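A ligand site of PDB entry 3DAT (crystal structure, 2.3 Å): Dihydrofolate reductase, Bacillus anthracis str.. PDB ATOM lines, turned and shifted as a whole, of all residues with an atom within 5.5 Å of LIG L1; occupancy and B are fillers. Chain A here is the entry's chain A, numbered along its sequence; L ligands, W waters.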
ATOM      1  N   MET A   6      15.878   9.035   2.927  1.00  0.00           N
ATOM      2  CA  MET A   6      16.950   8.124   3.306  1.00  0.00           C
ATOM      3  C   MET A   6      17.099   7.150   2.155  1.00  0.00           C
ATOM      4  O   MET A   6      16.221   6.333   1.968  1.00  0.00           O
ATOM      5  CB  MET A   6      16.502   7.403   4.583  1.00  0.00           C
ATOM      6  CG  MET A   6      17.275   6.153   4.974  1.00  0.00           C
ATOM      7  SD  MET A   6      18.953   6.521   5.534  1.00  0.00           S
ATOM      8  CE  MET A   6      18.608   7.456   7.034  1.00  0.00           C
ATOM      9  N   VAL A   7      18.163   7.247   1.370  1.00  0.00           N
ATOM     10  CA  VAL A   7      18.417   6.345   0.226  1.00  0.00           C
ATOM     11  C   VAL A   7      19.919   5.822   0.125  1.00  0.00           C
ATOM     12  O   VAL A   7      20.859   6.537   0.475  1.00  0.00           O
ATOM     13  CB  VAL A   7      18.019   7.046  -1.084  1.00  0.00           C
ATOM     14  CG1 VAL A   7      18.794   8.382  -1.279  1.00  0.00           C
ATOM     15  CG2 VAL A   7      18.154   6.108  -2.307  1.00  0.00           C
ATOM     16  N   ALA A   8      20.109   4.580  -0.320  1.00  0.00           N
ATOM     17  CA  ALA A   8      21.423   4.110  -0.790  1.00  0.00           C
ATOM     18  C   ALA A   8      21.405   4.078  -2.310  1.00  0.00           C
ATOM     19  O   ALA A   8      20.441   3.567  -2.887  1.00  0.00           O
ATOM     20  CB  ALA A   8      21.726   2.750  -0.247  1.00  0.00           C
ATOM     21  N   ASN A  20      14.525  -5.794  -4.873  1.00  0.00           N
ATOM     22  CA  ASN A  20      15.594  -6.046  -3.929  1.00  0.00           C
ATOM     23  C   ASN A  20      16.756  -5.127  -4.225  1.00  0.00           C
ATOM     24  O   ASN A  20      16.857  -4.552  -5.322  1.00  0.00           O
ATOM     25  CB  ASN A  20      16.080  -7.509  -4.070  1.00  0.00           C
ATOM     26  CG  ASN A  20      15.639  -8.380  -2.911  1.00  0.00           C
ATOM     27  OD1 ASN A  20      15.640  -7.965  -1.738  1.00  0.00           O
ATOM     28  ND2 ASN A  20      15.304  -9.632  -3.222  1.00  0.00           N
ATOM     29  N   LEU A  21      17.645  -4.983  -3.253  1.00  0.00           N
ATOM     30  CA  LEU A  21      18.886  -4.264  -3.456  1.00  0.00           C
ATOM     31  C   LEU A  21      19.745  -5.066  -4.420  1.00  0.00           C
ATOM     32  O   LEU A  21      19.802  -6.282  -4.317  1.00  0.00           O
ATOM     33  CB  LEU A  21      19.646  -4.131  -2.145  1.00  0.00           C
ATOM     34  CG  LEU A  21      18.869  -3.519  -0.992  1.00  0.00           C
ATOM     35  CD1 LEU A  21      19.606  -3.824   0.312  1.00  0.00           C
ATOM     36  CD2 LEU A  21      18.722  -2.027  -1.252  1.00  0.00           C
ATOM     37  N   TRP A  23      22.804  -5.106  -4.263  1.00  0.00           N
ATOM     38  CA  TRP A  23      23.994  -5.419  -3.462  1.00  0.00           C
ATOM     39  C   TRP A  23      23.583  -6.008  -2.098  1.00  0.00           C
ATOM     40  O   TRP A  23      22.401  -6.043  -1.755  1.00  0.00           O
ATOM     41  CB  TRP A  23      24.817  -4.153  -3.250  1.00  0.00           C
ATOM     42  CG  TRP A  23      23.994  -3.039  -2.702  1.00  0.00           C
ATOM     43  CD1 TRP A  23      23.638  -2.839  -1.401  1.00  0.00           C
ATOM     44  CD2 TRP A  23      23.383  -1.971  -3.448  1.00  0.00           C
ATOM     45  NE1 TRP A  23      22.863  -1.699  -1.279  1.00  0.00           N
ATOM     46  CE2 TRP A  23      22.697  -1.152  -2.528  1.00  0.00           C
ATOM     47  CE3 TRP A  23      23.376  -1.619  -4.800  1.00  0.00           C
ATOM     48  CZ2 TRP A  23      21.993  -0.011  -2.916  1.00  0.00           C
ATOM     49  CZ3 TRP A  23      22.679  -0.480  -5.181  1.00  0.00           C
ATOM     50  CH2 TRP A  23      21.997   0.305  -4.246  1.00  0.00           C
ATOM     51  N   PRO A  26      26.019  -5.438   4.766  1.00  0.00           N
ATOM     52  CA  PRO A  26      25.445  -5.430   6.130  1.00  0.00           C
ATOM     53  C   PRO A  26      25.825  -4.217   6.986  1.00  0.00           C
ATOM     54  O   PRO A  26      25.050  -3.809   7.844  1.00  0.00           O
ATOM     55  CB  PRO A  26      26.007  -6.716   6.762  1.00  0.00           C
ATOM     56  CG  PRO A  26      27.233  -7.056   5.952  1.00  0.00           C
ATOM     57  CD  PRO A  26      26.911  -6.587   4.548  1.00  0.00           C
ATOM     58  N   GLU A  28      26.193  -1.166   5.875  1.00  0.00           N
ATOM     59  CA  GLU A  28      25.415  -0.019   5.389  1.00  0.00           C
ATOM     60  C   GLU A  28      24.132   0.070   6.193  1.00  0.00           C
ATOM     61  O   GLU A  28      23.645   1.163   6.481  1.00  0.00           O
ATOM     62  CB  GLU A  28      25.081  -0.165   3.891  1.00  0.00           C
ATOM     63  CG  GLU A  28      24.791   1.172   3.163  1.00  0.00           C
ATOM     64  CD  GLU A  28      23.293   1.545   3.052  1.00  0.00           C
ATOM     65  OE1 GLU A  28      22.482   0.753   2.491  1.00  0.00           O
ATOM     66  OE2 GLU A  28      22.947   2.694   3.461  1.00  0.00           O
ATOM     67  N   LEU A  29      23.607  -1.102   6.539  1.00  0.00           N
ATOM     68  CA  LEU A  29      22.313  -1.224   7.183  1.00  0.00           C
ATOM     69  C   LEU A  29      22.345  -0.667   8.590  1.00  0.00           C
ATOM     70  O   LEU A  29      21.308  -0.453   9.203  1.00  0.00           O
ATOM     71  CB  LEU A  29      21.827  -2.686   7.188  1.00  0.00           C
ATOM     72  CG  LEU A  29      21.509  -3.188   5.768  1.00  0.00           C
ATOM     73  CD1 LEU A  29      21.046  -4.644   5.739  1.00  0.00           C
ATOM     74  CD2 LEU A  29      20.505  -2.296   5.071  1.00  0.00           C
ATOM     75  N   GLN A  30      23.538  -0.356   9.065  1.00  0.00           N
ATOM     76  CA  GLN A  30      23.773  -0.066  10.500  1.00  0.00           C
ATOM     77  C   GLN A  30      23.926   1.425  10.714  1.00  0.00           C
ATOM     78  O   GLN A  30      23.613   1.936  11.787  1.00  0.00           O
ATOM     79  CB  GLN A  30      25.012  -0.807  10.982  1.00  0.00           C
ATOM     80  CG  GLN A  30      24.840  -2.326  11.001  1.00  0.00           C
ATOM     81  CD  GLN A  30      23.969  -2.824  12.148  1.00  0.00           C
ATOM     82  OE1 GLN A  30      23.878  -2.207  13.227  1.00  0.00           O
ATOM     83  NE2 GLN A  30      23.340  -3.983  11.940  1.00  0.00           N
ATOM     84  N   VAL A  32      22.245   3.218   8.827  1.00  0.00           N
ATOM     85  CA  VAL A  32      20.833   3.405   8.501  1.00  0.00           C
ATOM     86  C   VAL A  32      19.998   3.122   9.731  1.00  0.00           C
ATOM     87  O   VAL A  32      19.089   3.856  10.027  1.00  0.00           O
ATOM     88  CB  VAL A  32      20.450   2.379   7.394  1.00  0.00           C
ATOM     89  CG1 VAL A  32      19.020   1.913   7.538  1.00  0.00           C
ATOM     90  CG2 VAL A  32      20.717   2.945   6.045  1.00  0.00           C
ATOM     91  N   LYS A  33      20.346   2.036  10.421  1.00  0.00           N
ATOM     92  CA  LYS A  33      19.681   1.642  11.631  1.00  0.00           C
ATOM     93  C   LYS A  33      19.823   2.738  12.687  1.00  0.00           C
ATOM     94  O   LYS A  33      18.830   3.127  13.282  1.00  0.00           O
ATOM     95  CB  LYS A  33      20.258   0.317  12.154  1.00  0.00           C
ATOM     96  CG  LYS A  33      19.640  -0.140  13.455  1.00  0.00           C
ATOM     97  CD  LYS A  33      20.152  -1.505  13.901  1.00  0.00           C
ATOM     98  CE  LYS A  33      19.220  -1.986  15.040  1.00  0.00           C
ATOM     99  NZ  LYS A  33      19.368  -3.466  15.289  1.00  0.00           N
ATOM    100  N   ASN A  47       8.773  -1.745  -1.395  1.00  0.00           N
ATOM    101  CA  ASN A  47       9.895  -1.702  -0.459  1.00  0.00           C
ATOM    102  C   ASN A  47       9.696  -2.661   0.689  1.00  0.00           C
ATOM    103  O   ASN A  47      10.493  -3.562   0.880  1.00  0.00           O
ATOM    104  CB  ASN A  47      10.119  -0.299   0.095  1.00  0.00           C
ATOM    105  CG  ASN A  47      11.435  -0.182   0.805  1.00  0.00           C
ATOM    106  OD1 ASN A  47      12.265  -1.077   0.716  1.00  0.00           O
ATOM    107  ND2 ASN A  47      11.650   0.936   1.493  1.00  0.00           N
ATOM    108  N   ALA A  50      10.281  -6.202   0.256  1.00  0.00           N
ATOM    109  CA  ALA A  50      11.716  -6.455   0.070  1.00  0.00           C
ATOM    110  C   ALA A  50      12.453  -6.573   1.413  1.00  0.00           C
ATOM    111  O   ALA A  50      13.612  -6.965   1.442  1.00  0.00           O
ATOM    112  CB  ALA A  50      12.346  -5.309  -0.811  1.00  0.00           C
ATOM    113  N   ILE A  51      11.765  -6.200   2.500  1.00  0.00           N
ATOM    114  CA  ILE A  51      12.299  -6.269   3.877  1.00  0.00           C
ATOM    115  C   ILE A  51      11.625  -7.406   4.634  1.00  0.00           C
ATOM    116  O   ILE A  51      12.247  -8.057   5.446  1.00  0.00           O
ATOM    117  CB  ILE A  51      12.098  -4.920   4.641  1.00  0.00           C
ATOM    118  CG1 ILE A  51      12.942  -3.807   4.027  1.00  0.00           C
ATOM    119  CG2 ILE A  51      12.437  -5.065   6.107  1.00  0.00           C
ATOM    120  CD1 ILE A  51      12.429  -2.370   4.254  1.00  0.00           C
ATOM    121  N   ARG A  53       9.621  -7.747   7.079  1.00  0.00           N
ATOM    122  CA  ARG A  53       9.421  -7.725   8.533  1.00  0.00           C
ATOM    123  C   ARG A  53       9.496  -6.311   9.088  1.00  0.00           C
ATOM    124  O   ARG A  53      10.168  -5.465   8.487  1.00  0.00           O
ATOM    125  CB  ARG A  53      10.475  -8.603   9.244  1.00  0.00           C
ATOM    126  CG  ARG A  53      11.902  -8.326   8.785  1.00  0.00           C
ATOM    127  CD  ARG A  53      12.938  -8.566   9.874  1.00  0.00           C
ATOM    128  NE  ARG A  53      14.074  -7.658   9.683  1.00  0.00           N
ATOM    129  CZ  ARG A  53      14.865  -7.229  10.659  1.00  0.00           C
ATOM    130  NH1 ARG A  53      14.680  -7.637  11.908  1.00  0.00           N
ATOM    131  NH2 ARG A  53      15.850  -6.383  10.381  1.00  0.00           N
ATOM    132  N   LEU A  55      10.901  -3.391  11.332  1.00  0.00           N
ATOM    133  CA  LEU A  55      12.224  -3.036  11.839  1.00  0.00           C
ATOM    134  C   LEU A  55      12.085  -2.411  13.228  1.00  0.00           C
ATOM    135  O   LEU A  55      11.410  -1.405  13.414  1.00  0.00           O
ATOM    136  CB  LEU A  55      12.874  -2.037  10.871  1.00  0.00           C
ATOM    137  CG  LEU A  55      13.677  -2.535   9.656  1.00  0.00           C
ATOM    138  CD1 LEU A  55      13.486  -4.032   9.338  1.00  0.00           C
ATOM    139  CD2 LEU A  55      13.378  -1.703   8.459  1.00  0.00           C
ATOM    140  N   PRO A  56      12.715  -3.026  14.251  1.00  0.00           N
ATOM    141  CA  PRO A  56      12.428  -2.569  15.618  1.00  0.00           C
ATOM    142  C   PRO A  56      12.822  -1.118  15.931  1.00  0.00           C
ATOM    143  O   PRO A  56      13.647  -0.524  15.214  1.00  0.00           O
ATOM    144  CB  PRO A  56      13.218  -3.560  16.470  1.00  0.00           C
ATOM    145  CG  PRO A  56      13.380  -4.758  15.591  1.00  0.00           C
ATOM    146  CD  PRO A  56      13.649  -4.163  14.248  1.00  0.00           C
ATOM    147  N   ARG A  58      11.232   1.684  15.622  1.00  0.00           N
ATOM    148  CA  ARG A  58      10.689   2.745  14.785  1.00  0.00           C
ATOM    149  C   ARG A  58       9.252   2.379  14.421  1.00  0.00           C
ATOM    150  O   ARG A  58       8.915   1.204  14.328  1.00  0.00           O
ATOM    151  CB  ARG A  58      11.542   2.892  13.513  1.00  0.00           C
ATOM    152  CG  ARG A  58      12.966   3.397  13.760  1.00  0.00           C
ATOM    153  CD  ARG A  58      13.989   2.710  12.873  1.00  0.00           C
ATOM    154  NE  ARG A  58      14.396   1.376  13.355  1.00  0.00           N
ATOM    155  CZ  ARG A  58      15.263   0.582  12.733  1.00  0.00           C
ATOM    156  NH1 ARG A  58      15.862   0.975  11.599  1.00  0.00           N
ATOM    157  NH2 ARG A  58      15.561  -0.597  13.249  1.00  0.00           N
ATOM    158  N   ILE A  95      11.545   9.095   4.950  1.00  0.00           N
ATOM    159  CA  ILE A  95      11.058   8.463   3.761  1.00  0.00           C
ATOM    160  C   ILE A  95      12.103   7.452   3.372  1.00  0.00           C
ATOM    161  O   ILE A  95      13.236   7.815   3.001  1.00  0.00           O
ATOM    162  CB  ILE A  95      10.772   9.495   2.636  1.00  0.00           C
ATOM    163  CG1 ILE A  95      10.070  10.721   3.243  1.00  0.00           C
ATOM    164  CG2 ILE A  95       9.934   8.850   1.489  1.00  0.00           C
ATOM    165  CD1 ILE A  95       8.737  10.453   4.006  1.00  0.00           C
ATOM    166  N   PHE A  96      11.714   6.190   3.511  1.00  0.00           N
ATOM    167  CA  PHE A  96      12.623   5.071   3.438  1.00  0.00           C
ATOM    168  C   PHE A  96      12.503   4.485   2.049  1.00  0.00           C
ATOM    169  O   PHE A  96      13.067   3.434   1.732  1.00  0.00           O
ATOM    170  CB  PHE A  96      12.210   4.040   4.471  1.00  0.00           C
ATOM    171  CG  PHE A  96      13.313   3.209   4.941  1.00  0.00           C
ATOM    172  CD1 PHE A  96      14.449   3.798   5.479  1.00  0.00           C
ATOM    173  CD2 PHE A  96      13.220   1.827   4.870  1.00  0.00           C
ATOM    174  CE1 PHE A  96      15.500   3.014   5.941  1.00  0.00           C
ATOM    175  CE2 PHE A  96      14.262   1.020   5.348  1.00  0.00           C
ATOM    176  CZ  PHE A  96      15.413   1.620   5.875  1.00  0.00           C
ATOM    177  N   GLY A  97      11.705   5.150   1.237  1.00  0.00           N
ATOM    178  CA  GLY A  97      11.681   4.866  -0.155  1.00  0.00           C
ATOM    179  C   GLY A  97      10.936   3.691  -0.677  1.00  0.00           C
ATOM    180  O   GLY A  97      10.080   3.123  -0.022  1.00  0.00           O
ATOM    181  N   TYR A 102       9.475   8.049  -2.983  1.00  0.00           N
ATOM    182  CA  TYR A 102      10.313   9.228  -2.990  1.00  0.00           C
ATOM    183  C   TYR A 102       9.540  10.256  -3.833  1.00  0.00           C
ATOM    184  O   TYR A 102       9.369  11.379  -3.412  1.00  0.00           O
ATOM    185  CB  TYR A 102      11.763   8.969  -3.538  1.00  0.00           C
ATOM    186  CG  TYR A 102      12.632   8.089  -2.658  1.00  0.00           C
ATOM    187  CD1 TYR A 102      12.890   8.420  -1.329  1.00  0.00           C
ATOM    188  CD2 TYR A 102      13.237   6.932  -3.169  1.00  0.00           C
ATOM    189  CE1 TYR A 102      13.697   7.619  -0.509  1.00  0.00           C
ATOM    190  CE2 TYR A 102      14.045   6.117  -2.381  1.00  0.00           C
ATOM    191  CZ  TYR A 102      14.267   6.450  -1.046  1.00  0.00           C
ATOM    192  OH  TYR A 102      15.052   5.616  -0.256  1.00  0.00           O
ATOM    193  N   TYR A 113      19.526  11.935   3.085  1.00  0.00           N
ATOM    194  CA  TYR A 113      20.556  11.002   3.579  1.00  0.00           C
ATOM    195  C   TYR A 113      20.869   9.996   2.518  1.00  0.00           C
ATOM    196  O   TYR A 113      20.122   9.041   2.310  1.00  0.00           O
ATOM    197  CB  TYR A 113      20.116  10.291   4.852  1.00  0.00           C
ATOM    198  CG  TYR A 113      19.857  11.225   5.995  1.00  0.00           C
ATOM    199  CD1 TYR A 113      18.656  11.931   6.094  1.00  0.00           C
ATOM    200  CD2 TYR A 113      20.797  11.403   6.985  1.00  0.00           C
ATOM    201  CE1 TYR A 113      18.408  12.790   7.150  1.00  0.00           C
ATOM    202  CE2 TYR A 113      20.564  12.261   8.041  1.00  0.00           C
ATOM    203  CZ  TYR A 113      19.376  12.952   8.109  1.00  0.00           C
ATOM    204  OH  TYR A 113      19.170  13.788   9.162  1.00  0.00           O
ATOM    205  N   THR A 115      23.739   7.478   0.618  1.00  0.00           N
ATOM    206  CA  THR A 115      24.909   6.676   0.547  1.00  0.00           C
ATOM    207  C   THR A 115      25.204   6.591  -0.930  1.00  0.00           C
ATOM    208  O   THR A 115      24.302   6.360  -1.733  1.00  0.00           O
ATOM    209  CB  THR A 115      24.605   5.293   1.129  1.00  0.00           C
ATOM    210  OG1 THR A 115      24.345   5.420   2.545  1.00  0.00           O
ATOM    211  CG2 THR A 115      25.748   4.356   0.935  1.00  0.00           C
HETATM  212  N1  LIG L   1      20.087   2.244   2.648  1.00  0.00           N
HETATM  213  C1  LIG L   1      19.804   3.558   2.741  1.00  0.00           C
HETATM  214  N2  LIG L   1      20.825   4.355   2.874  1.00  0.00           N
HETATM  215  N3  LIG L   1      18.488   4.023   2.710  1.00  0.00           N
HETATM  216  C2  LIG L   1      17.452   3.135   2.579  1.00  0.00           C
HETATM  217  N4  LIG L   1      16.196   3.580   2.431  1.00  0.00           N
HETATM  218  C3  LIG L   1      17.747   1.774   2.462  1.00  0.00           C
HETATM  219  N5  LIG L   1      16.743   0.842   2.331  1.00  0.00           N
HETATM  220  C4  LIG L   1      17.039  -0.499   2.219  1.00  0.00           C
HETATM  221  C5  LIG L   1      18.365  -0.935   2.249  1.00  0.00           C
HETATM  222  N6  LIG L   1      19.388  -0.009   2.402  1.00  0.00           N
HETATM  223  C6  LIG L   1      19.072   1.336   2.506  1.00  0.00           C
HETATM  224  C7  LIG L   1      15.886  -1.443   2.054  1.00  0.00           C
HETATM  225  N7  LIG L   1      16.191  -2.834   2.309  1.00  0.00           N
HETATM  226  C8  LIG L   1      15.789  -3.750   1.224  1.00  0.00           C
HETATM  227  C9  LIG L   1      17.059  -4.175   6.254  1.00  0.00           C
HETATM  228  C10 LIG L   1      16.907  -5.125   5.236  1.00  0.00           C
HETATM  229  C11 LIG L   1      16.606  -4.691   3.941  1.00  0.00           C
HETATM  230  C12 LIG L   1      16.487  -3.308   3.652  1.00  0.00           C
HETATM  231  C13 LIG L   1      16.671  -2.385   4.689  1.00  0.00           C
HETATM  232  C14 LIG L   1      16.786  -2.822   6.015  1.00  0.00           C
HETATM  233  C15 LIG L   1      17.396  -4.546   7.673  1.00  0.00           C
HETATM  234  O1  LIG L   1      17.074  -5.818   8.219  1.00  0.00           O
HETATM  235  N8  LIG L   1      18.056  -3.627   8.367  1.00  0.00           N
HETATM  236  C16 LIG L   1      18.134  -3.675   9.809  1.00  0.00           C
HETATM  237  C17 LIG L   1      17.406  -2.508  10.409  1.00  0.00           C
HETATM  238  O2  LIG L   1      17.593  -1.344   9.984  1.00  0.00           O
HETATM  239  O3  LIG L   1      16.599  -2.689  11.351  1.00  0.00           O
HETATM  240  C18 LIG L   1      19.591  -3.765  10.289  1.00  0.00           C
HETATM  241  C19 LIG L   1      20.270  -5.084   9.886  1.00  0.00           C
HETATM  242  C20 LIG L   1      19.494  -6.341  10.285  1.00  0.00           C
HETATM  243  O4  LIG L   1      18.689  -6.324  11.255  1.00  0.00           O
HETATM  244  O5  LIG L   1      19.670  -7.421   9.664  1.00  0.00           O
HETATM  245  P1  LG2 L   2       7.894   1.367  -3.689  1.00  0.00           P
HETATM  246  O1  LG2 L   2       7.836   2.855  -3.865  1.00  0.00           O
HETATM  247  O2  LG2 L   2       8.786   0.948  -2.574  1.00  0.00           O
HETATM  248  O3  LG2 L   2       6.413   0.886  -3.363  1.00  0.00           O
HETATM  249  C1  LG2 L   2       5.457   1.112  -4.364  1.00  0.00           C
HETATM  250  C2  LG2 L   2       4.062   0.915  -3.814  1.00  0.00           C
HETATM  251  O4  LG2 L   2       3.664   2.045  -3.058  1.00  0.00           O
HETATM  252  C3  LG2 L   2       3.040   0.878  -4.953  1.00  0.00           C
HETATM  253  O5  LG2 L   2       3.068  -0.368  -5.611  1.00  0.00           O
HETATM  254  C4  LG2 L   2       1.770   1.188  -4.181  1.00  0.00           C
HETATM  255  O6  LG2 L   2       1.380   0.050  -3.422  1.00  0.00           O
HETATM  256  C5  LG2 L   2       2.255   2.207  -3.172  1.00  0.00           C
HETATM  257  N1  LG2 L   2       1.870   3.527  -3.692  1.00  0.00           N
HETATM  258  C6  LG2 L   2       2.410   4.187  -4.766  1.00  0.00           C
HETATM  259  N2  LG2 L   2       1.712   5.347  -4.904  1.00  0.00           N
HETATM  260  C7  LG2 L   2       0.762   5.420  -3.953  1.00  0.00           C
HETATM  261  C8  LG2 L   2      -0.213   6.374  -3.659  1.00  0.00           C
HETATM  262  N3  LG2 L   2      -0.322   7.510  -4.375  1.00  0.00           N
HETATM  263  N4  LG2 L   2      -1.070   6.167  -2.580  1.00  0.00           N
HETATM  264  C9  LG2 L   2      -0.972   5.005  -1.834  1.00  0.00           C
HETATM  265  N5  LG2 L   2      -0.015   4.070  -2.162  1.00  0.00           N
HETATM  266  C10 LG2 L   2       0.847   4.276  -3.190  1.00  0.00           C
HETATM  267  O7  LG2 L   2       8.237   0.699  -5.097  1.00  0.00           O
HETATM  268  P2  LG2 L   2       9.470   0.846  -6.122  1.00  0.00           P
HETATM  269  O8  LG2 L   2       9.410   2.160  -6.777  1.00  0.00           O
HETATM  270  O9  LG2 L   2       9.463  -0.324  -6.976  1.00  0.00           O
HETATM  271  O10 LG2 L   2      10.757   0.723  -5.190  1.00  0.00           O
HETATM  272  C11 LG2 L   2      11.069  -0.540  -4.669  1.00  0.00           C
HETATM  273  C12 LG2 L   2      12.421  -1.020  -5.204  1.00  0.00           C
HETATM  274  O11 LG2 L   2      13.433  -0.122  -4.826  1.00  0.00           O
HETATM  275  C13 LG2 L   2      12.844  -2.375  -4.631  1.00  0.00           C
HETATM  276  O12 LG2 L   2      13.761  -2.969  -5.534  1.00  0.00           O
HETATM  277  C14 LG2 L   2      13.581  -1.959  -3.386  1.00  0.00           C
HETATM  278  O13 LG2 L   2      14.512  -2.928  -2.977  1.00  0.00           O
HETATM  279  C15 LG2 L   2      14.296  -0.710  -3.871  1.00  0.00           C
HETATM  280  N6  LG2 L   2      14.642   0.221  -2.786  1.00  0.00           N
HETATM  281  C16 LG2 L   2      15.960   0.528  -2.579  1.00  0.00           C
HETATM  282  C17 LG2 L   2      16.326   1.409  -1.555  1.00  0.00           C
HETATM  283  C18 LG2 L   2      17.730   1.863  -1.442  1.00  0.00           C
HETATM  284  O14 LG2 L   2      18.046   2.921  -0.558  1.00  0.00           O
HETATM  285  N7  LG2 L   2      18.641   1.253  -2.219  1.00  0.00           N
HETATM  286  C19 LG2 L   2      15.354   1.970  -0.764  1.00  0.00           C
HETATM  287  C20 LG2 L   2      14.013   1.637  -0.985  1.00  0.00           C
HETATM  288  C21 LG2 L   2      13.662   0.764  -2.007  1.00  0.00           C
HETATM  289  P3  LG2 L   2       0.147  -0.898  -3.875  1.00  0.00           P
HETATM  290  O15 LG2 L   2      -0.044  -1.860  -2.763  1.00  0.00           O
HETATM  291  O16 LG2 L   2      -1.114  -0.114  -4.074  1.00  0.00           O
HETATM  292  O17 LG2 L   2       0.524  -1.457  -5.229  1.00  0.00           O
HETATM  293  O   HOH W   1      21.398   6.833   3.022  1.00  0.00           O
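O of Val 7 sits at hydrogen-bond distance from N2 of LIG L1. The backbone NH (N) of Ala 8 is in hydrogen-bond range of an oxygen (O14) of LG2 L2, 2.7 Å away. N4 of LIG L1 sits at hydrogen-bond distance from O of Met 6 (2.8 Å). The backbone NH (N) of Asn 20 lies within hydrogen-bond range of an oxygen (O12) of LG2 L2, at 3.0 Å. An oxygen (O2) of LG2 L2 sits at hydrogen-bond distance from the backbone NH (N) of Asn 47 (2.9 Å). The backbone carbonyl oxygen (O) of Phe 96 sits at hydrogen-bond distance from a nitrogen (N4) of LIG L1, at 3.2 Å. The backbone carbonyl oxygen (O) of Ala 8 sits at hydrogen-bond distance from a nitrogen (N7) of LG2 L2, at 3.0 Å. A nitrogen (N2) of LIG L1 is in hydrogen-bond range of the side-chain carboxylate (OE2) of Glu 28 (2.8 Å). NH2 of Arg 53 is in salt-bridge range of O4 of LIG L1 (3.0 Å). A nitrogen (N3) of LIG L1 lies close to the backbone NH (N) of Ala 8 (3.5 Å). O of Asn 20 sits at hydrogen-bond distance from O12 of LG2 L2, 3.5 Å away. NH2 of Arg 58 lies within salt-bridge range of O3 of LIG L1 (3.0 Å).
O of Met 6 lies within hydrogen-bond range of OH of Tyr 102, at 2.6 Å. The guanidinium group (NH2) of Arg 58 sits at hydrogen-bond distance from the backbone carbonyl oxygen (O) of Pro 56, 2.7 Å away. The backbone NH (N) of Val 7 lies within hydrogen-bond range of the backbone carbonyl oxygen (O) of Tyr 113 (2.8 Å). OG1 of Thr 115 lies within hydrogen-bond range of OE2 of Glu 28 (3.2 Å). The backbone carbonyl oxygen of Gly 97 sits at hydrogen-bond distance from the side-chain amide nitrogen of Asn 47, 3.1 Å away. The backbone carbonyl oxygen of Phe 96 lies within hydrogen-bond range of the side-chain amide nitrogen of Asn 47. The backbone carbonyl oxygen (O) of Val 7 is in hydrogen-bond range of the backbone NH (N) of Thr 115. The backbone NH (N) of Met 6 is in hydrogen-bond range of the backbone carbonyl oxygen (O) of Ile 95, 2.9 Å away.
Residues that only touch LIG L1: Leu 21 (3.7 Å), Leu 29 (3.7 Å), Gln 30 (3.9 Å), Val 32 (3.5 Å), Lys 33 (3.8 Å), Asn 47 (3.9 Å), Ala 50 (3.9 Å), Ile 51 (3.6 Å), Leu 55 (3.4 Å), Tyr 102 (3.6 Å) and Thr 115 (3.7 Å). Hydrophobic or aromatic side chains that line LIG L1: Met 6, Ala 8, Leu 21, Leu 29, Val 32, Ile 51, Leu 55 and Phe 96. Within 4 Å of LIG L1: Met 6, Val 7, Ala 8, Leu 21, Glu 28, Leu 29, Gln 30, Val 32, Lys 33, Asn 47, Ala 50, Ile 51, Arg 53, Leu 55, Arg 58, Phe 96, Tyr 102 and Thr 115. The nearest printed residue that does not touch LIG L1 is Pro 56 (4.4 Å).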
